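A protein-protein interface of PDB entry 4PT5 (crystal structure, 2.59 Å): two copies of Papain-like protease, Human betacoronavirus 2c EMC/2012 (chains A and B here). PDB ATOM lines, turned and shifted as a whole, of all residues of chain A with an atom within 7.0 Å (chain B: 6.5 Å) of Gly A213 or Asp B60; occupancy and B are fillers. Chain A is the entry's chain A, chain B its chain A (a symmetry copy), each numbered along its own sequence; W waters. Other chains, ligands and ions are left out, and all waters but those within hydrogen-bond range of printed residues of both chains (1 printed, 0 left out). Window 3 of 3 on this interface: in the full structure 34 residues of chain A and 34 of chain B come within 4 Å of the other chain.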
ATOM      1  N   TYR A 211     -19.721  16.520 -30.672  1.00  0.00           N
ATOM      2  CA  TYR A 211     -20.282  16.696 -29.334  1.00  0.00           C
ATOM      3  C   TYR A 211     -20.335  15.373 -28.580  1.00  0.00           C
ATOM      4  O   TYR A 211     -20.750  14.347 -29.125  1.00  0.00           O
ATOM      5  CB  TYR A 211     -21.681  17.318 -29.393  1.00  0.00           C
ATOM      6  CG  TYR A 211     -22.208  17.772 -28.045  1.00  0.00           C
ATOM      7  CD1 TYR A 211     -22.857  16.880 -27.189  1.00  0.00           C
ATOM      8  CD2 TYR A 211     -22.059  19.096 -27.626  1.00  0.00           C
ATOM      9  CE1 TYR A 211     -23.334  17.291 -25.955  1.00  0.00           C
ATOM     10  CE2 TYR A 211     -22.537  19.516 -26.393  1.00  0.00           C
ATOM     11  CZ  TYR A 211     -23.175  18.611 -25.563  1.00  0.00           C
ATOM     12  OH  TYR A 211     -23.651  19.020 -24.338  1.00  0.00           O
ATOM     13  N   VAL A 212     -19.915  15.412 -27.320  1.00  0.00           N
ATOM     14  CA  VAL A 212     -19.952  14.247 -26.446  1.00  0.00           C
ATOM     15  C   VAL A 212     -20.906  14.513 -25.282  1.00  0.00           C
ATOM     16  O   VAL A 212     -20.784  15.524 -24.586  1.00  0.00           O
ATOM     17  CB  VAL A 212     -18.544  13.889 -25.925  1.00  0.00           C
ATOM     18  CG1 VAL A 212     -18.571  12.577 -25.154  1.00  0.00           C
ATOM     19  CG2 VAL A 212     -17.564  13.793 -27.084  1.00  0.00           C
ATOM     20  N   GLY A 213     -21.859  13.604 -25.089  1.00  0.00           N
ATOM     21  CA  GLY A 213     -22.861  13.737 -24.037  1.00  0.00           C
ATOM     22  C   GLY A 213     -24.219  13.215 -24.465  1.00  0.00           C
ATOM     23  O   GLY A 213     -24.837  12.416 -23.759  1.00  0.00           O
ATOM     24  N   VAL A 214     -24.679  13.680 -25.624  1.00  0.00           N
ATOM     25  CA  VAL A 214     -25.950  13.246 -26.205  1.00  0.00           C
ATOM     26  C   VAL A 214     -25.708  12.475 -27.499  1.00  0.00           C
ATOM     27  O   VAL A 214     -24.670  12.644 -28.143  1.00  0.00           O
ATOM     28  CB  VAL A 214     -26.909  14.432 -26.468  1.00  0.00           C
ATOM     29  CG1 VAL A 214     -27.404  15.021 -25.156  1.00  0.00           C
ATOM     30  CG2 VAL A 214     -26.239  15.497 -27.324  1.00  0.00           C
ATOM     31  N   GLN A 215     -26.666  11.629 -27.871  1.00  0.00           N
ATOM     32  CA  GLN A 215     -26.539  10.785 -29.060  1.00  0.00           C
ATOM     33  C   GLN A 215     -27.660  10.997 -30.085  1.00  0.00           C
ATOM     34  O   GLN A 215     -27.625  10.421 -31.176  1.00  0.00           O
ATOM     35  CB  GLN A 215     -26.427   9.314 -28.661  1.00  0.00           C
ATOM     36  CG  GLN A 215     -25.102   8.966 -28.002  1.00  0.00           C
ATOM     37  CD  GLN A 215     -25.109   7.595 -27.357  1.00  0.00           C
ATOM     38  OE1 GLN A 215     -26.015   7.259 -26.596  1.00  0.00           O
ATOM     39  NE2 GLN A 215     -24.089   6.800 -27.648  1.00  0.00           N
ATOM     40  N   ASP A 219     -32.052  15.631 -28.347  1.00  0.00           N
ATOM     41  CA  ASP A 219     -31.456  15.823 -27.028  1.00  0.00           C
ATOM     42  C   ASP A 219     -30.433  16.957 -27.026  1.00  0.00           C
ATOM     43  O   ASP A 219     -30.310  17.679 -26.041  1.00  0.00           O
ATOM     44  CB  ASP A 219     -30.812  14.526 -26.536  1.00  0.00           C
ATOM     45  CG  ASP A 219     -31.831  13.427 -26.269  1.00  0.00           C
ATOM     46  OD1 ASP A 219     -33.041  13.727 -26.188  1.00  0.00           O
ATOM     47  OD2 ASP A 219     -31.417  12.256 -26.141  1.00  0.00           O
ATOM     48  N   LEU A 248     -21.937  12.788 -33.014  1.00  0.00           N
ATOM     49  CA  LEU A 248     -22.309  12.757 -31.601  1.00  0.00           C
ATOM     50  C   LEU A 248     -21.788  11.480 -30.951  1.00  0.00           C
ATOM     51  O   LEU A 248     -21.847  10.405 -31.548  1.00  0.00           O
ATOM     52  CB  LEU A 248     -23.829  12.846 -31.428  1.00  0.00           C
ATOM     53  CG  LEU A 248     -24.620  14.038 -31.980  1.00  0.00           C
ATOM     54  CD1 LEU A 248     -26.101  13.840 -31.699  1.00  0.00           C
ATOM     55  CD2 LEU A 248     -24.154  15.365 -31.402  1.00  0.00           C
ATOM     56  N   SER A 249     -21.281  11.602 -29.727  1.00  0.00           N
ATOM     57  CA  SER A 249     -20.714  10.461 -29.017  1.00  0.00           C
ATOM     58  C   SER A 249     -21.245  10.324 -27.595  1.00  0.00           C
ATOM     59  O   SER A 249     -21.649  11.303 -26.967  1.00  0.00           O
ATOM     60  CB  SER A 249     -19.186  10.544 -28.991  1.00  0.00           C
ATOM     61  OG  SER A 249     -18.647  10.485 -30.298  1.00  0.00           O
ATOM     62  N   GLY A 250     -21.231   9.090 -27.107  1.00  0.00           N
ATOM     63  CA  GLY A 250     -21.608   8.760 -25.740  1.00  0.00           C
ATOM     64  C   GLY A 250     -21.082   7.373 -25.424  1.00  0.00           C
ATOM     65  O   GLY A 250     -20.554   6.689 -26.305  1.00  0.00           O
ATOM     66  N   THR A 251     -21.218   6.953 -24.171  1.00  0.00           N
ATOM     67  CA  THR A 251     -20.792   5.613 -23.771  1.00  0.00           C
ATOM     68  C   THR A 251     -21.790   4.577 -24.298  1.00  0.00           C
ATOM     69  O   THR A 251     -22.908   4.941 -24.669  1.00  0.00           O
ATOM     70  CB  THR A 251     -20.630   5.487 -22.238  1.00  0.00           C
ATOM     71  OG1 THR A 251     -21.886   5.729 -21.591  1.00  0.00           O
ATOM     72  CG2 THR A 251     -19.580   6.472 -21.720  1.00  0.00           C
ATOM     73  N   ARG B  18     -22.355  22.964  -8.576  1.00  0.00           N
ATOM     74  CA  ARG B  18     -23.673  23.490  -8.936  1.00  0.00           C
ATOM     75  C   ARG B  18     -24.774  22.541  -8.480  1.00  0.00           C
ATOM     76  O   ARG B  18     -24.569  21.324  -8.421  1.00  0.00           O
ATOM     77  CB  ARG B  18     -23.778  23.774 -10.440  1.00  0.00           C
ATOM     78  CG  ARG B  18     -23.598  22.570 -11.352  1.00  0.00           C
ATOM     79  CD  ARG B  18     -23.606  23.019 -12.801  1.00  0.00           C
ATOM     80  NE  ARG B  18     -23.260  21.946 -13.732  1.00  0.00           N
ATOM     81  CZ  ARG B  18     -24.143  21.209 -14.400  1.00  0.00           C
ATOM     82  NH1 ARG B  18     -25.448  21.404 -14.247  1.00  0.00           N
ATOM     83  NH2 ARG B  18     -23.717  20.268 -15.228  1.00  0.00           N
ATOM     84  N   ARG B  29     -28.390   9.744 -17.018  1.00  0.00           N
ATOM     85  CA  ARG B  29     -27.847  10.010 -18.349  1.00  0.00           C
ATOM     86  C   ARG B  29     -28.665  11.041 -19.128  1.00  0.00           C
ATOM     87  O   ARG B  29     -28.103  11.964 -19.722  1.00  0.00           O
ATOM     88  CB  ARG B  29     -27.772   8.705 -19.143  1.00  0.00           C
ATOM     89  CG  ARG B  29     -27.035   8.803 -20.465  1.00  0.00           C
ATOM     90  CD  ARG B  29     -27.271   7.557 -21.298  1.00  0.00           C
ATOM     91  NE  ARG B  29     -26.170   7.324 -22.226  1.00  0.00           N
ATOM     92  CZ  ARG B  29     -25.090   6.601 -21.942  1.00  0.00           C
ATOM     93  NH1 ARG B  29     -24.956   6.026 -20.753  1.00  0.00           N
ATOM     94  NH2 ARG B  29     -24.140   6.455 -22.854  1.00  0.00           N
ATOM     95  N   LEU B  32     -28.752  14.560 -16.626  1.00  0.00           N
ATOM     96  CA  LEU B  32     -27.478  15.272 -16.506  1.00  0.00           C
ATOM     97  C   LEU B  32     -26.486  14.843 -17.582  1.00  0.00           C
ATOM     98  O   LEU B  32     -26.158  15.616 -18.485  1.00  0.00           O
ATOM     99  CB  LEU B  32     -26.854  15.033 -15.128  1.00  0.00           C
ATOM    100  CG  LEU B  32     -27.072  16.039 -13.999  1.00  0.00           C
ATOM    101  CD1 LEU B  32     -26.680  15.401 -12.677  1.00  0.00           C
ATOM    102  CD2 LEU B  32     -26.278  17.318 -14.241  1.00  0.00           C
ATOM    103  N   GLY B  33     -26.013  13.606 -17.465  1.00  0.00           N
ATOM    104  CA  GLY B  33     -25.009  13.051 -18.366  1.00  0.00           C
ATOM    105  C   GLY B  33     -24.251  11.934 -17.681  1.00  0.00           C
ATOM    106  O   GLY B  33     -24.814  11.202 -16.865  1.00  0.00           O
ATOM    107  N   CYS B  34     -22.968  11.804 -18.006  1.00  0.00           N
ATOM    108  CA  CYS B  34     -22.128  10.788 -17.391  1.00  0.00           C
ATOM    109  C   CYS B  34     -21.707  11.212 -15.984  1.00  0.00           C
ATOM    110  O   CYS B  34     -20.879  12.109 -15.816  1.00  0.00           O
ATOM    111  CB  CYS B  34     -20.907  10.489 -18.265  1.00  0.00           C
ATOM    112  SG  CYS B  34     -20.150   8.882 -17.929  1.00  0.00           S
ATOM    113  N   VAL B  35     -22.288  10.565 -14.978  1.00  0.00           N
ATOM    114  CA  VAL B  35     -22.031  10.918 -13.578  1.00  0.00           C
ATOM    115  C   VAL B  35     -21.379   9.798 -12.771  1.00  0.00           C
ATOM    116  O   VAL B  35     -21.701   8.618 -12.944  1.00  0.00           O
ATOM    117  CB  VAL B  35     -23.309  11.403 -12.852  1.00  0.00           C
ATOM    118  CG1 VAL B  35     -23.721  12.778 -13.352  1.00  0.00           C
ATOM    119  CG2 VAL B  35     -24.447  10.402 -13.006  1.00  0.00           C
ATOM    120  N   SER B  43     -24.610   6.376 -14.478  1.00  0.00           N
ATOM    121  CA  SER B  43     -25.282   7.139 -15.535  1.00  0.00           C
ATOM    122  C   SER B  43     -26.626   6.550 -15.963  1.00  0.00           C
ATOM    123  O   SER B  43     -27.579   7.291 -16.214  1.00  0.00           O
ATOM    124  CB  SER B  43     -24.368   7.280 -16.756  1.00  0.00           C
ATOM    125  OG  SER B  43     -23.135   7.880 -16.402  1.00  0.00           O
ATOM    126  N   LEU B  58     -19.200  14.850 -12.823  1.00  0.00           N
ATOM    127  CA  LEU B  58     -19.769  14.836 -14.172  1.00  0.00           C
ATOM    128  C   LEU B  58     -18.690  14.739 -15.253  1.00  0.00           C
ATOM    129  O   LEU B  58     -17.614  15.314 -15.115  1.00  0.00           O
ATOM    130  CB  LEU B  58     -20.617  16.097 -14.374  1.00  0.00           C
ATOM    131  CG  LEU B  58     -21.404  16.322 -15.665  1.00  0.00           C
ATOM    132  CD1 LEU B  58     -22.690  15.510 -15.686  1.00  0.00           C
ATOM    133  CD2 LEU B  58     -21.708  17.802 -15.826  1.00  0.00           C
ATOM    134  N   ALA B  59     -18.993  14.016 -16.329  1.00  0.00           N
ATOM    135  CA  ALA B  59     -18.039  13.805 -17.423  1.00  0.00           C
ATOM    136  C   ALA B  59     -18.573  14.263 -18.781  1.00  0.00           C
ATOM    137  O   ALA B  59     -17.797  14.476 -19.714  1.00  0.00           O
ATOM    138  CB  ALA B  59     -17.619  12.344 -17.486  1.00  0.00           C
ATOM    139  N   ASP B  60     -19.894  14.410 -18.878  1.00  0.00           N
ATOM    140  CA  ASP B  60     -20.569  14.793 -20.120  1.00  0.00           C
ATOM    141  C   ASP B  60     -21.375  16.075 -19.951  1.00  0.00           C
ATOM    142  O   ASP B  60     -21.660  16.491 -18.828  1.00  0.00           O
ATOM    143  CB  ASP B  60     -21.512  13.675 -20.573  1.00  0.00           C
ATOM    144  CG  ASP B  60     -20.790  12.539 -21.270  1.00  0.00           C
ATOM    145  OD1 ASP B  60     -19.598  12.692 -21.613  1.00  0.00           O
ATOM    146  OD2 ASP B  60     -21.426  11.484 -21.484  1.00  0.00           O
ATOM    147  N   ASN B  61     -21.746  16.686 -21.077  1.00  0.00           N
ATOM    148  CA  ASN B  61     -22.613  17.871 -21.102  1.00  0.00           C
ATOM    149  C   ASN B  61     -22.181  18.980 -20.140  1.00  0.00           C
ATOM    150  O   ASN B  61     -23.004  19.557 -19.427  1.00  0.00           O
ATOM    151  CB  ASN B  61     -24.072  17.478 -20.843  1.00  0.00           C
ATOM    152  CG  ASN B  61     -24.580  16.442 -21.823  1.00  0.00           C
ATOM    153  OD1 ASN B  61     -24.586  16.661 -23.036  1.00  0.00           O
ATOM    154  ND2 ASN B  61     -25.015  15.301 -21.300  1.00  0.00           N
ATOM    155  N   LEU B  62     -20.884  19.266 -20.125  1.00  0.00           N
ATOM    156  CA  LEU B  62     -20.343  20.276 -19.227  1.00  0.00           C
ATOM    157  C   LEU B  62     -20.816  21.672 -19.624  1.00  0.00           C
ATOM    158  O   LEU B  62     -20.925  21.995 -20.810  1.00  0.00           O
ATOM    159  CB  LEU B  62     -18.812  20.234 -19.201  1.00  0.00           C
ATOM    160  CG  LEU B  62     -18.048  18.921 -18.993  1.00  0.00           C
ATOM    161  CD1 LEU B  62     -16.598  19.244 -18.671  1.00  0.00           C
ATOM    162  CD2 LEU B  62     -18.647  18.047 -17.901  1.00  0.00           C
ATOM    163  N   THR B  63     -21.105  22.486 -18.616  1.00  0.00           N
ATOM    164  CA  THR B  63     -21.465  23.881 -18.825  1.00  0.00           C
ATOM    165  C   THR B  63     -20.219  24.678 -19.220  1.00  0.00           C
ATOM    166  O   THR B  63     -19.093  24.219 -19.007  1.00  0.00           O
ATOM    167  CB  THR B  63     -22.108  24.481 -17.562  1.00  0.00           C
ATOM    168  OG1 THR B  63     -21.251  24.262 -16.435  1.00  0.00           O
ATOM    169  CG2 THR B  63     -23.456  23.829 -17.291  1.00  0.00           C
ATOM    170  N   GLU B  66     -17.899  24.876 -16.475  1.00  0.00           N
ATOM    171  CA  GLU B  66     -17.270  23.585 -16.194  1.00  0.00           C
ATOM    172  C   GLU B  66     -16.172  23.246 -17.202  1.00  0.00           C
ATOM    173  O   GLU B  66     -15.109  22.762 -16.818  1.00  0.00           O
ATOM    174  CB  GLU B  66     -18.318  22.469 -16.143  1.00  0.00           C
ATOM    175  CG  GLU B  66     -19.077  22.406 -14.826  1.00  0.00           C
ATOM    176  CD  GLU B  66     -20.248  21.439 -14.851  1.00  0.00           C
ATOM    177  OE1 GLU B  66     -20.804  21.181 -15.941  1.00  0.00           O
ATOM    178  OE2 GLU B  66     -20.622  20.944 -13.765  1.00  0.00           O
ATOM    179  N   PRO B  79     -12.272  14.704 -25.094  1.00  0.00           N
ATOM    180  CA  PRO B  79     -13.530  14.631 -24.331  1.00  0.00           C
ATOM    181  C   PRO B  79     -13.868  13.274 -23.671  1.00  0.00           C
ATOM    182  O   PRO B  79     -14.926  13.157 -23.048  1.00  0.00           O
ATOM    183  CB  PRO B  79     -14.594  15.019 -25.365  1.00  0.00           C
ATOM    184  CG  PRO B  79     -13.987  14.685 -26.683  1.00  0.00           C
ATOM    185  CD  PRO B  79     -12.513  14.919 -26.536  1.00  0.00           C
ATOM    186  N   LEU B  82     -12.083  12.442 -18.781  1.00  0.00           N
ATOM    187  CA  LEU B  82     -12.663  12.357 -17.440  1.00  0.00           C
ATOM    188  C   LEU B  82     -13.176  10.959 -17.109  1.00  0.00           C
ATOM    189  O   LEU B  82     -12.801  10.391 -16.082  1.00  0.00           O
ATOM    190  CB  LEU B  82     -13.768  13.396 -17.246  1.00  0.00           C
ATOM    191  CG  LEU B  82     -13.339  14.838 -16.962  1.00  0.00           C
ATOM    192  CD1 LEU B  82     -14.558  15.744 -16.905  1.00  0.00           C
ATOM    193  CD2 LEU B  82     -12.533  14.938 -15.673  1.00  0.00           C
ATOM    194  N   HIS B  83     -14.019  10.404 -17.980  1.00  0.00           N
ATOM    195  CA  HIS B  83     -14.530   9.045 -17.796  1.00  0.00           C
ATOM    196  C   HIS B  83     -13.399   8.067 -17.659  1.00  0.00           C
ATOM    197  O   HIS B  83     -13.458   7.142 -16.848  1.00  0.00           O
ATOM    198  CB  HIS B  83     -15.435   8.634 -18.955  1.00  0.00           C
ATOM    199  CG  HIS B  83     -16.047   7.260 -18.789  1.00  0.00           C
ATOM    200  ND1 HIS B  83     -15.325   6.127 -18.898  1.00  0.00           N
ATOM    201  CD2 HIS B  83     -17.354   6.867 -18.511  1.00  0.00           C
ATOM    202  CE1 HIS B  83     -16.125   5.064 -18.697  1.00  0.00           C
ATOM    203  NE2 HIS B  83     -17.368   5.517 -18.462  1.00  0.00           N
HETATM  204  O   HOH W   1     -19.632  18.198 -22.667  1.00  0.00           O
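Among the printed residues, merely in contact across the chains: Val A212 with Asp B60 (3.7 Å), Val A212 with Asn B61 (3.8 Å), Val A212 with Pro B79 (3.6 Å), Gly A213 with Asp B60 (3.7 Å), Gly A213 with Asn B61 (3.5 Å), Val A214 with Asn B61 (3.9 Å) and Thr A251 with His B83 (3.9 Å).
O of Tyr A211 sits at hydrogen-bond distance from N of Ser A249 (2.9 Å). N of Gly A213 sits at hydrogen-bond distance from O of Ser A249, 3.0 Å away. The backbone carbonyl oxygen (O) of Ser B43 is in hydrogen-bond range of the backbone NH (N) of Arg B29 (2.7 Å). O of Leu B32 is in hydrogen-bond range of ND2 of Asn B61 (3.1 Å).
O of Thr A251 is in hydrogen-bond range of NH2 of Arg B29. The side-chain hydroxyl (OH) of Tyr A211 lies within hydrogen-bond range of the side-chain amide oxygen (OD1) of Asn B61 (2.9 Å).
Along chain A the printed residues that touch a printed residue of chain B span positions 211 to 251. Among the printed residues, 9 pairs touch across the chains.
No position is printed for both chains. Of the 9 pairs that touch across the chains among the printed residues, none has its exchanged pair printed and touching as well.
Water W1 lies within hydrogen-bond range of N of Leu B62 (3.0 Å), N of Asn B61 (3.0 Å) and O of Val A212 (3.5 Å).
Of chain B, only Asp B60 (3.7 Å) and Asn B61 (3.5 Å) come within 4 Å of Gly A213. Asp B60 touches just these residues of chain A: Val A212 (3.7 Å) and Gly A213 (3.7 Å). Printed residues of chain A within 4 Å of Pro B79: Val A212. Of the printed residues of chain B, Thr A251 touches Arg B29 and His B83. Of the printed residues of chain A, Arg B29 touches Thr A251 (2.7 Å). Leu B62 touches none of the printed residues of chain A. The nearest residue of chain A that does not touch Asp B60 is Gly A250 (5.1 Å).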
